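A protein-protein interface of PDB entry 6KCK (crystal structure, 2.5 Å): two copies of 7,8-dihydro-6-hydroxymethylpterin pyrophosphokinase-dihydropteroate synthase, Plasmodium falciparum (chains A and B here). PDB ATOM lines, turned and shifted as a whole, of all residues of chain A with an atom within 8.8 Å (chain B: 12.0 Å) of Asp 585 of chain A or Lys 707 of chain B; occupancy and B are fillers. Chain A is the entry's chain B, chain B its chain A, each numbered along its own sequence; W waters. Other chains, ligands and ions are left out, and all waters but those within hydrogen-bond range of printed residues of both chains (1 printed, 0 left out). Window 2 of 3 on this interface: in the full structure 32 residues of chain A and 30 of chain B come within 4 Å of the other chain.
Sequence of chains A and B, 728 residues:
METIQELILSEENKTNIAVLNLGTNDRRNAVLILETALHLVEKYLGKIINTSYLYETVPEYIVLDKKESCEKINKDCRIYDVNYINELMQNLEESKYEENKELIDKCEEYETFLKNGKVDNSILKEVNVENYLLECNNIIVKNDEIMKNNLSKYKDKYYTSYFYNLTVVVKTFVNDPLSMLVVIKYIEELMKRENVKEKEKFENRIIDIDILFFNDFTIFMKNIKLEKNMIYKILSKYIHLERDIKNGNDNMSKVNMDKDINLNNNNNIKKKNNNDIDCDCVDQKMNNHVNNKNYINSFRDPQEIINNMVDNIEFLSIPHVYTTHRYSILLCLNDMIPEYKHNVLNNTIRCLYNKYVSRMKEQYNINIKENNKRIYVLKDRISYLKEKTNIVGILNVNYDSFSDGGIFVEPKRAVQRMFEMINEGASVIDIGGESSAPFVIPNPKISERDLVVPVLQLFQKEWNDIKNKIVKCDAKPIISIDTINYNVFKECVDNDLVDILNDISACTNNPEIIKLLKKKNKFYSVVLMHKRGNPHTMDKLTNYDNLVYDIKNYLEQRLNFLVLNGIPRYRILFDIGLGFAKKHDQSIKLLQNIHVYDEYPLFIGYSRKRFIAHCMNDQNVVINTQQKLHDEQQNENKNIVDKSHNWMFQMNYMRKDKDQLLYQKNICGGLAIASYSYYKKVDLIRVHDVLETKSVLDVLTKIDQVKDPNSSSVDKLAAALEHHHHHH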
ATOM      1  N   LEU A 547      -2.756  24.356  -9.992  1.00  0.00           N
ATOM      2  CA  LEU A 547      -2.520  25.540  -9.163  1.00  0.00           C
ATOM      3  C   LEU A 547      -1.071  26.087  -9.213  1.00  0.00           C
ATOM      4  O   LEU A 547      -0.825  27.193  -9.666  1.00  0.00           O
ATOM      5  CB  LEU A 547      -2.935  25.220  -7.704  1.00  0.00           C
ATOM      6  CG  LEU A 547      -2.604  26.321  -6.691  1.00  0.00           C
ATOM      7  CD1 LEU A 547      -3.507  27.556  -6.838  1.00  0.00           C
ATOM      8  CD2 LEU A 547      -2.545  25.805  -5.252  1.00  0.00           C
ATOM      9  N   VAL A 548      -0.126  25.299  -8.727  1.00  0.00           N
ATOM     10  CA  VAL A 548       1.263  25.695  -8.646  1.00  0.00           C
ATOM     11  C   VAL A 548       1.822  26.160  -9.969  1.00  0.00           C
ATOM     12  O   VAL A 548       2.417  27.219 -10.057  1.00  0.00           O
ATOM     13  CB  VAL A 548       2.118  24.556  -8.032  1.00  0.00           C
ATOM     14  CG1 VAL A 548       3.612  24.861  -8.146  1.00  0.00           C
ATOM     15  CG2 VAL A 548       1.729  24.389  -6.593  1.00  0.00           C
ATOM     16  N   LEU A 578      -0.645  35.130  -2.269  1.00  0.00           N
ATOM     17  CA  LEU A 578      -1.389  34.399  -1.235  1.00  0.00           C
ATOM     18  C   LEU A 578      -2.672  35.138  -0.869  1.00  0.00           C
ATOM     19  O   LEU A 578      -2.658  36.343  -0.649  1.00  0.00           O
ATOM     20  CB  LEU A 578      -0.552  34.201   0.012  1.00  0.00           C
ATOM     21  CG  LEU A 578       0.802  33.533  -0.228  1.00  0.00           C
ATOM     22  CD1 LEU A 578       1.660  33.746   0.998  1.00  0.00           C
ATOM     23  CD2 LEU A 578       0.573  32.054  -0.523  1.00  0.00           C
ATOM     24  N   LYS A 582      -7.420  32.308  -3.824  1.00  0.00           N
ATOM     25  CA  LYS A 582      -6.938  31.010  -3.419  1.00  0.00           C
ATOM     26  C   LYS A 582      -7.706  30.619  -2.181  1.00  0.00           C
ATOM     27  O   LYS A 582      -7.864  31.427  -1.289  1.00  0.00           O
ATOM     28  CB  LYS A 582      -5.432  31.030  -3.088  1.00  0.00           C
ATOM     29  CG  LYS A 582      -4.490  31.067  -4.281  1.00  0.00           C
ATOM     30  CD  LYS A 582      -3.875  32.448  -4.498  1.00  0.00           C
ATOM     31  CE  LYS A 582      -3.449  32.598  -5.944  1.00  0.00           C
ATOM     32  NZ  LYS A 582      -3.015  33.967  -6.379  1.00  0.00           N
ATOM     33  N   LYS A 583      -8.165  29.377  -2.093  1.00  0.00           N
ATOM     34  CA  LYS A 583      -8.675  28.896  -0.821  1.00  0.00           C
ATOM     35  C   LYS A 583      -7.482  28.763   0.119  1.00  0.00           C
ATOM     36  O   LYS A 583      -6.326  28.692  -0.327  1.00  0.00           O
ATOM     37  CB  LYS A 583      -9.460  27.584  -0.966  1.00  0.00           C
ATOM     38  CG  LYS A 583     -10.642  27.710  -1.935  1.00  0.00           C
ATOM     39  CD  LYS A 583     -11.838  26.908  -1.468  1.00  0.00           C
ATOM     40  CE  LYS A 583     -12.999  26.952  -2.466  1.00  0.00           C
ATOM     41  NZ  LYS A 583     -13.950  28.103  -2.308  1.00  0.00           N
ATOM     42  N   HIS A 584      -7.760  28.738   1.415  1.00  0.00           N
ATOM     43  CA  HIS A 584      -6.692  28.642   2.414  1.00  0.00           C
ATOM     44  C   HIS A 584      -5.757  27.492   2.219  1.00  0.00           C
ATOM     45  O   HIS A 584      -4.543  27.676   2.330  1.00  0.00           O
ATOM     46  CB  HIS A 584      -7.253  28.714   3.822  1.00  0.00           C
ATOM     47  CG  HIS A 584      -8.114  29.920   4.038  1.00  0.00           C
ATOM     48  ND1 HIS A 584      -7.971  31.072   3.284  1.00  0.00           N
ATOM     49  CD2 HIS A 584      -9.150  30.161   4.946  1.00  0.00           C
ATOM     50  CE1 HIS A 584      -8.869  31.979   3.696  1.00  0.00           C
ATOM     51  NE2 HIS A 584      -9.585  31.426   4.724  1.00  0.00           N
ATOM     52  N   ASP A 585      -6.298  26.326   1.873  1.00  0.00           N
ATOM     53  CA  ASP A 585      -5.448  25.155   1.519  1.00  0.00           C
ATOM     54  C   ASP A 585      -4.623  25.365   0.238  1.00  0.00           C
ATOM     55  O   ASP A 585      -3.555  24.771   0.087  1.00  0.00           O
ATOM     56  CB  ASP A 585      -6.245  23.835   1.437  1.00  0.00           C
ATOM     57  CG  ASP A 585      -6.677  23.299   2.828  1.00  0.00           C
ATOM     58  OD1 ASP A 585      -5.829  23.135   3.742  1.00  0.00           O
ATOM     59  OD2 ASP A 585      -7.887  23.020   3.018  1.00  0.00           O
ATOM     60  N   GLN A 586      -5.098  26.227  -0.654  1.00  0.00           N
ATOM     61  CA  GLN A 586      -4.347  26.575  -1.854  1.00  0.00           C
ATOM     62  C   GLN A 586      -3.192  27.546  -1.576  1.00  0.00           C
ATOM     63  O   GLN A 586      -2.103  27.426  -2.154  1.00  0.00           O
ATOM     64  CB  GLN A 586      -5.281  27.112  -2.938  1.00  0.00           C
ATOM     65  CG  GLN A 586      -6.194  26.069  -3.559  1.00  0.00           C
ATOM     66  CD  GLN A 586      -7.251  26.695  -4.461  1.00  0.00           C
ATOM     67  OE1 GLN A 586      -7.789  27.761  -4.145  1.00  0.00           O
ATOM     68  NE2 GLN A 586      -7.519  26.071  -5.594  1.00  0.00           N
ATOM     69  N   SER A 587      -3.435  28.513  -0.701  1.00  0.00           N
ATOM     70  CA  SER A 587      -2.372  29.348  -0.195  1.00  0.00           C
ATOM     71  C   SER A 587      -1.251  28.502   0.468  1.00  0.00           C
ATOM     72  O   SER A 587      -0.062  28.691   0.184  1.00  0.00           O
ATOM     73  CB  SER A 587      -2.957  30.371   0.779  1.00  0.00           C
ATOM     74  OG  SER A 587      -3.675  31.380   0.078  1.00  0.00           O
ATOM     75  N   ILE A 588      -1.621  27.533   1.301  1.00  0.00           N
ATOM     76  CA  ILE A 588      -0.626  26.664   1.954  1.00  0.00           C
ATOM     77  C   ILE A 588       0.132  25.895   0.890  1.00  0.00           C
ATOM     78  O   ILE A 588       1.373  25.758   0.943  1.00  0.00           O
ATOM     79  CB  ILE A 588      -1.281  25.672   2.926  1.00  0.00           C
ATOM     80  CG1 ILE A 588      -2.003  26.404   4.070  1.00  0.00           C
ATOM     81  CG2 ILE A 588      -0.279  24.653   3.455  1.00  0.00           C
ATOM     82  CD1 ILE A 588      -1.079  27.310   4.843  1.00  0.00           C
ATOM     83  N   LYS A 589      -0.609  25.421  -0.104  1.00  0.00           N
ATOM     84  CA  LYS A 589      -0.020  24.615  -1.128  1.00  0.00           C
ATOM     85  C   LYS A 589       1.018  25.394  -1.956  1.00  0.00           C
ATOM     86  O   LYS A 589       2.075  24.836  -2.365  1.00  0.00           O
ATOM     87  CB  LYS A 589      -1.091  23.994  -2.017  1.00  0.00           C
ATOM     88  CG  LYS A 589      -0.481  22.900  -2.887  1.00  0.00           C
ATOM     89  CD  LYS A 589      -1.519  21.997  -3.516  1.00  0.00           C
ATOM     90  CE  LYS A 589      -0.807  20.895  -4.296  1.00  0.00           C
ATOM     91  NZ  LYS A 589      -1.786  20.360  -5.286  1.00  0.00           N
ATOM     92  N   LEU A 590       0.719  26.671  -2.191  1.00  0.00           N
ATOM     93  CA  LEU A 590       1.632  27.543  -2.874  1.00  0.00           C
ATOM     94  C   LEU A 590       2.914  27.707  -2.042  1.00  0.00           C
ATOM     95  O   LEU A 590       3.988  27.689  -2.601  1.00  0.00           O
ATOM     96  CB  LEU A 590       0.966  28.894  -3.151  1.00  0.00           C
ATOM     97  CG  LEU A 590      -0.002  28.850  -4.335  1.00  0.00           C
ATOM     98  CD1 LEU A 590      -0.783  30.143  -4.400  1.00  0.00           C
ATOM     99  CD2 LEU A 590       0.711  28.579  -5.657  1.00  0.00           C
ATOM    100  N   LEU A 591       2.783  27.900  -0.731  1.00  0.00           N
ATOM    101  CA  LEU A 591       3.931  27.844   0.211  1.00  0.00           C
ATOM    102  C   LEU A 591       4.672  26.496   0.223  1.00  0.00           C
ATOM    103  O   LEU A 591       5.900  26.478   0.135  1.00  0.00           O
ATOM    104  CB  LEU A 591       3.515  28.219   1.640  1.00  0.00           C
ATOM    105  CG  LEU A 591       3.201  29.709   1.847  1.00  0.00           C
ATOM    106  CD1 LEU A 591       2.520  29.949   3.191  1.00  0.00           C
ATOM    107  CD2 LEU A 591       4.472  30.550   1.723  1.00  0.00           C
ATOM    108  N   GLN A 592       3.932  25.384   0.288  1.00  0.00           N
ATOM    109  CA  GLN A 592       4.591  24.054   0.274  1.00  0.00           C
ATOM    110  C   GLN A 592       5.498  23.900  -0.957  1.00  0.00           C
ATOM    111  O   GLN A 592       6.536  23.226  -0.894  1.00  0.00           O
ATOM    112  CB  GLN A 592       3.578  22.910   0.307  1.00  0.00           C
ATOM    113  CG  GLN A 592       2.801  22.875   1.604  1.00  0.00           C
ATOM    114  CD  GLN A 592       1.676  21.841   1.633  1.00  0.00           C
ATOM    115  OE1 GLN A 592       1.132  21.497   0.593  1.00  0.00           O
ATOM    116  NE2 GLN A 592       1.308  21.359   2.844  1.00  0.00           N
ATOM    117  N   ASN A 593       5.115  24.561  -2.059  1.00  0.00           N
ATOM    118  CA  ASN A 593       5.760  24.370  -3.333  1.00  0.00           C
ATOM    119  C   ASN A 593       6.491  25.606  -3.786  1.00  0.00           C
ATOM    120  O   ASN A 593       6.711  25.830  -4.980  1.00  0.00           O
ATOM    121  CB  ASN A 593       4.710  23.931  -4.357  1.00  0.00           C
ATOM    122  CG  ASN A 593       4.225  22.519  -4.107  1.00  0.00           C
ATOM    123  OD1 ASN A 593       4.913  21.581  -4.442  1.00  0.00           O
ATOM    124  ND2 ASN A 593       3.052  22.366  -3.512  1.00  0.00           N
ATOM    125  N   ARG A 610      -6.215  35.513   6.090  1.00  0.00           N
ATOM    126  CA  ARG A 610      -7.107  34.590   6.721  1.00  0.00           C
ATOM    127  C   ARG A 610      -6.533  33.167   6.744  1.00  0.00           C
ATOM    128  O   ARG A 610      -6.776  32.413   7.696  1.00  0.00           O
ATOM    129  CB  ARG A 610      -8.458  34.620   5.981  1.00  0.00           C
ATOM    130  CG  ARG A 610      -9.190  35.980   5.988  1.00  0.00           C
ATOM    131  CD  ARG A 610     -10.254  36.072   4.883  1.00  0.00           C
ATOM    132  NE  ARG A 610      -9.666  36.101   3.542  1.00  0.00           N
ATOM    133  CZ  ARG A 610     -10.314  35.903   2.381  1.00  0.00           C
ATOM    134  NH1 ARG A 610     -11.612  35.632   2.340  1.00  0.00           N
ATOM    135  NH2 ARG A 610      -9.644  35.985   1.236  1.00  0.00           N
ATOM    136  N   PHE A 611      -5.754  32.779   5.723  1.00  0.00           N
ATOM    137  CA  PHE A 611      -5.261  31.393   5.675  1.00  0.00           C
ATOM    138  C   PHE A 611      -4.371  31.009   6.863  1.00  0.00           C
ATOM    139  O   PHE A 611      -4.198  29.812   7.129  1.00  0.00           O
ATOM    140  CB  PHE A 611      -4.553  31.057   4.343  1.00  0.00           C
ATOM    141  CG  PHE A 611      -3.125  31.519   4.269  1.00  0.00           C
ATOM    142  CD1 PHE A 611      -2.815  32.811   3.817  1.00  0.00           C
ATOM    143  CD2 PHE A 611      -2.090  30.673   4.678  1.00  0.00           C
ATOM    144  CE1 PHE A 611      -1.487  33.245   3.768  1.00  0.00           C
ATOM    145  CE2 PHE A 611      -0.775  31.099   4.613  1.00  0.00           C
ATOM    146  CZ  PHE A 611      -0.464  32.387   4.159  1.00  0.00           C
ATOM    147  N   ILE A 612      -3.788  32.003   7.535  1.00  0.00           N
ATOM    148  CA  ILE A 612      -3.003  31.733   8.746  1.00  0.00           C
ATOM    149  C   ILE A 612      -3.878  31.172   9.883  1.00  0.00           C
ATOM    150  O   ILE A 612      -3.527  30.155  10.502  1.00  0.00           O
ATOM    151  CB  ILE A 612      -2.243  32.964   9.258  1.00  0.00           C
ATOM    152  CG1 ILE A 612      -1.179  33.425   8.260  1.00  0.00           C
ATOM    153  CG2 ILE A 612      -1.526  32.616  10.547  1.00  0.00           C
ATOM    154  CD1 ILE A 612      -0.569  34.769   8.611  1.00  0.00           C
ATOM    155  N   HIS A 614      -6.597  29.655   9.602  1.00  0.00           N
ATOM    156  CA  HIS A 614      -6.980  28.327   9.134  1.00  0.00           C
ATOM    157  C   HIS A 614      -5.984  27.270   9.528  1.00  0.00           C
ATOM    158  O   HIS A 614      -6.295  26.077   9.497  1.00  0.00           O
ATOM    159  CB  HIS A 614      -7.158  28.383   7.607  1.00  0.00           C
ATOM    160  CG  HIS A 614      -7.669  27.103   6.985  1.00  0.00           C
ATOM    161  ND1 HIS A 614      -6.843  26.205   6.401  1.00  0.00           N
ATOM    162  CD2 HIS A 614      -8.980  26.593   6.842  1.00  0.00           C
ATOM    163  CE1 HIS A 614      -7.581  25.158   5.919  1.00  0.00           C
ATOM    164  NE2 HIS A 614      -8.886  25.401   6.191  1.00  0.00           N
ATOM    165  N   CYS A 615      -4.769  27.677   9.882  1.00  0.00           N
ATOM    166  CA  CYS A 615      -3.752  26.716  10.362  1.00  0.00           C
ATOM    167  C   CYS A 615      -3.879  26.324  11.845  1.00  0.00           C
ATOM    168  O   CYS A 615      -3.335  25.314  12.265  1.00  0.00           O
ATOM    169  CB  CYS A 615      -2.346  27.212  10.051  1.00  0.00           C
ATOM    170  SG  CYS A 615      -2.045  27.405   8.271  1.00  0.00           S
ATOM    171  N   ASP B 698       1.774  25.094  15.070  1.00  0.00           N
ATOM    172  CA  ASP B 698       0.603  24.758  14.258  1.00  0.00           C
ATOM    173  C   ASP B 698       0.806  25.182  12.807  1.00  0.00           C
ATOM    174  O   ASP B 698       0.583  24.396  11.864  1.00  0.00           O
ATOM    175  CB  ASP B 698      -0.661  25.408  14.827  1.00  0.00           C
ATOM    176  CG  ASP B 698      -1.261  24.622  15.991  1.00  0.00           C
ATOM    177  OD1 ASP B 698      -0.777  23.520  16.365  1.00  0.00           O
ATOM    178  OD2 ASP B 698      -2.248  25.122  16.553  1.00  0.00           O
ATOM    179  N   VAL B 699       1.269  26.409  12.606  1.00  0.00           N
ATOM    180  CA  VAL B 699       1.483  26.824  11.233  1.00  0.00           C
ATOM    181  C   VAL B 699       2.495  25.925  10.537  1.00  0.00           C
ATOM    182  O   VAL B 699       2.239  25.484   9.424  1.00  0.00           O
ATOM    183  CB  VAL B 699       1.872  28.284  11.080  1.00  0.00           C
ATOM    184  CG1 VAL B 699       2.244  28.551   9.635  1.00  0.00           C
ATOM    185  CG2 VAL B 699       0.724  29.179  11.505  1.00  0.00           C
ATOM    186  N   LEU B 700       3.627  25.645  11.187  1.00  0.00           N
ATOM    187  CA  LEU B 700       4.703  24.935  10.526  1.00  0.00           C
ATOM    188  C   LEU B 700       4.315  23.485  10.268  1.00  0.00           C
ATOM    189  O   LEU B 700       4.785  22.860   9.298  1.00  0.00           O
ATOM    190  CB  LEU B 700       5.969  24.976  11.383  1.00  0.00           C
ATOM    191  CG  LEU B 700       6.650  26.325  11.655  1.00  0.00           C
ATOM    192  CD1 LEU B 700       7.860  26.113  12.539  1.00  0.00           C
ATOM    193  CD2 LEU B 700       7.075  27.020  10.375  1.00  0.00           C
ATOM    194  N   THR B 701       3.477  22.943  11.152  1.00  0.00           N
ATOM    195  CA  THR B 701       2.909  21.607  10.991  1.00  0.00           C
ATOM    196  C   THR B 701       1.963  21.564   9.752  1.00  0.00           C
ATOM    197  O   THR B 701       2.003  20.632   8.964  1.00  0.00           O
ATOM    198  CB  THR B 701       2.215  21.158  12.307  1.00  0.00           C
ATOM    199  OG1 THR B 701       3.176  21.194  13.380  1.00  0.00           O
ATOM    200  CG2 THR B 701       1.611  19.749  12.198  1.00  0.00           C
ATOM    201  N   LYS B 702       1.163  22.602   9.571  1.00  0.00           N
ATOM    202  CA  LYS B 702       0.256  22.715   8.441  1.00  0.00           C
ATOM    203  C   LYS B 702       1.066  22.771   7.142  1.00  0.00           C
ATOM    204  O   LYS B 702       0.832  21.984   6.202  1.00  0.00           O
ATOM    205  CB  LYS B 702      -0.649  23.943   8.628  1.00  0.00           C
ATOM    206  CG  LYS B 702      -1.853  24.031   7.698  1.00  0.00           C
ATOM    207  CD  LYS B 702      -3.121  23.481   8.338  1.00  0.00           C
ATOM    208  CE  LYS B 702      -3.531  22.165   7.691  1.00  0.00           C
ATOM    209  NZ  LYS B 702      -4.555  21.416   8.478  1.00  0.00           N
ATOM    210  N   ILE B 703       2.081  23.626   7.100  1.00  0.00           N
ATOM    211  CA  ILE B 703       2.937  23.664   5.909  1.00  0.00           C
ATOM    212  C   ILE B 703       3.528  22.306   5.533  1.00  0.00           C
ATOM    213  O   ILE B 703       3.711  22.018   4.336  1.00  0.00           O
ATOM    214  CB  ILE B 703       4.034  24.732   5.992  1.00  0.00           C
ATOM    215  CG1 ILE B 703       3.400  26.115   6.119  1.00  0.00           C
ATOM    216  CG2 ILE B 703       4.940  24.665   4.764  1.00  0.00           C
ATOM    217  CD1 ILE B 703       4.396  27.197   6.458  1.00  0.00           C
ATOM    218  N   ASP B 704       3.796  21.465   6.537  1.00  0.00           N
ATOM    219  CA  ASP B 704       4.398  20.154   6.297  1.00  0.00           C
ATOM    220  C   ASP B 704       3.416  19.062   5.905  1.00  0.00           C
ATOM    221  O   ASP B 704       3.823  18.083   5.345  1.00  0.00           O
ATOM    222  CB  ASP B 704       5.193  19.678   7.509  1.00  0.00           C
ATOM    223  CG  ASP B 704       6.599  20.223   7.529  1.00  0.00           C
ATOM    224  OD1 ASP B 704       7.077  20.749   6.485  1.00  0.00           O
ATOM    225  OD2 ASP B 704       7.229  20.127   8.602  1.00  0.00           O
ATOM    226  N   GLN B 705       2.143  19.229   6.218  1.00  0.00           N
ATOM    227  CA  GLN B 705       1.144  18.207   5.975  1.00  0.00           C
ATOM    228  C   GLN B 705       0.679  18.244   4.504  1.00  0.00           C
ATOM    229  O   GLN B 705      -0.068  19.136   4.096  1.00  0.00           O
ATOM    230  CB  GLN B 705      -0.014  18.422   6.967  1.00  0.00           C
ATOM    231  CG  GLN B 705      -1.379  17.851   6.602  1.00  0.00           C
ATOM    232  CD  GLN B 705      -2.537  18.699   7.160  1.00  0.00           C
ATOM    233  OE1 GLN B 705      -3.427  19.137   6.412  1.00  0.00           O
ATOM    234  NE2 GLN B 705      -2.519  18.946   8.477  1.00  0.00           N
ATOM    235  N   VAL B 706       1.134  17.299   3.690  1.00  0.00           N
ATOM    236  CA  VAL B 706       0.630  17.265   2.308  1.00  0.00           C
ATOM    237  C   VAL B 706      -0.767  16.615   2.219  1.00  0.00           C
ATOM    238  O   VAL B 706      -0.982  15.489   2.704  1.00  0.00           O
ATOM    239  CB  VAL B 706       1.644  16.682   1.297  1.00  0.00           C
ATOM    240  CG1 VAL B 706       1.103  16.803  -0.125  1.00  0.00           C
ATOM    241  CG2 VAL B 706       2.981  17.408   1.416  1.00  0.00           C
ATOM    242  N   LYS B 707      -1.705  17.367   1.627  1.00  0.00           N
ATOM    243  CA  LYS B 707      -3.116  16.975   1.507  1.00  0.00           C
ATOM    244  C   LYS B 707      -3.423  16.045   0.327  1.00  0.00           C
ATOM    245  O   LYS B 707      -2.905  16.228  -0.783  1.00  0.00           O
ATOM    246  CB  LYS B 707      -4.020  18.213   1.440  1.00  0.00           C
ATOM    247  CG  LYS B 707      -4.284  18.861   2.788  1.00  0.00           C
ATOM    248  CD  LYS B 707      -5.687  19.452   2.851  1.00  0.00           C
ATOM    249  CE  LYS B 707      -6.023  19.988   4.242  1.00  0.00           C
ATOM    250  NZ  LYS B 707      -6.157  18.925   5.283  1.00  0.00           N
ATOM    251  N   ASP B 708      -4.288  15.064   0.588  1.00  0.00           N
ATOM    252  CA  ASP B 708      -4.680  14.056  -0.408  1.00  0.00           C
ATOM    253  C   ASP B 708      -6.102  14.292  -0.927  1.00  0.00           C
ATOM    254  O   ASP B 708      -6.545  13.649  -1.882  1.00  0.00           O
ATOM    255  CB  ASP B 708      -4.559  12.643   0.182  1.00  0.00           C
ATOM    256  CG  ASP B 708      -3.128  12.282   0.552  1.00  0.00           C
ATOM    257  OD1 ASP B 708      -2.351  11.910  -0.358  1.00  0.00           O
ATOM    258  OD2 ASP B 708      -2.786  12.362   1.754  1.00  0.00           O
HETATM  259  O   HOH W   1      -1.489  20.972   4.706  1.00  0.00           O
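The side-chain amino group (NZ) of Lys 702 of chain B sits close to the side-chain amide nitrogen (NE2) of Gln 705 of chain B (3.2 Å). NZ of Lys 707 of chain B sits at hydrogen-bond distance from OE1 of Gln 705 of chain B (3.0 Å). SG of Cys 615 of chain A is in hydrogen-bond range of O of Phe 611 of chain A (3.4 Å).
Asp 585 of chain A touches one residue of chain B. Of chain A, only Asp 585 (3.2 Å) comes within 4 Å of Lys 707 of chain B. No residue of chain B comes within 4 Å of His 584 of chain A. No residue of chain B comes within 4 Å of Gln 586 of chain A. No residue of chain B comes within 4 Å of Ser 587 of chain A. Lys 589 of chain A touches none of the printed residues of chain B. No residue of chain A comes within 4 Å of Val 706 of chain B. Of the printed residues of chain A, Gln 705 of chain B touches Gln 592 (2.9 Å). Printed residues of chain A within 4 Å of Val 699 of chain B: Cys 615. Of the printed residues of chain A, Lys 702 of chain B touches Ile 588 (3.99 Å), Gln 592 (3.4 Å) and Cys 615 (3.4 Å). Of the printed residues of chain B, Gln 592 of chain A touches Lys 702, Ile 703 and Gln 705. Lys 583 of chain A touches none of the printed residues of chain B. Thr 701 of chain B touches none of the printed residues of chain A. The nearest residue of chain A that does not touch Lys 707 of chain B is Gln 592 of chain A (5.1 Å).
Among the printed residues, pairs that only touch across the chains: Asp 585 of chain A with Lys 707 of chain B (3.2 Å), Cys 615 of chain A with Lys 702 of chain B (3.4 Å), Cys 615 of chain A with Asp 698 of chain B (3.7 Å), Cys 615 of chain A with Val 699 of chain B (3.9 Å) and Ile 588 of chain A with Lys 702 of chain B (3.99 Å).
No position is printed for both chains. Of the 8 pairs that touch across the chains among the printed residues, none has its exchanged pair printed and touching as well.
The side-chain amide nitrogen of Gln 592 of chain A sits at hydrogen-bond distance from the backbone carbonyl oxygen of Lys 702 of chain B, 3.4 Å away. NE2 of Gln 592 of chain A is in hydrogen-bond range of O of Ile 703 of chain B, at 2.9 Å. The side-chain amide nitrogen (NE2) of Gln 592 of chain A sits at hydrogen-bond distance from the backbone carbonyl oxygen (O) of Gln 705 of chain B.
Of the 20 printed residues of chain A, 4 touch a printed residue of chain B. Printed residues of chain B that touch a printed residue of chain A: Asp 698, Val 699, Lys 702, Ile 703, Gln 705 and Lys 707. Hydrophobic or aromatic side chains of chain B within 4 Å of the printed part of chain A: Val 699. Among the printed residues, 8 pairs touch across the chains.
Water W1 lies within hydrogen-bond range of O of Gln 705 of chain B (2.4 Å), O of Lys 702 of chain B (2.9 Å) and NE2 of Gln 592 of chain A (3.4 Å).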
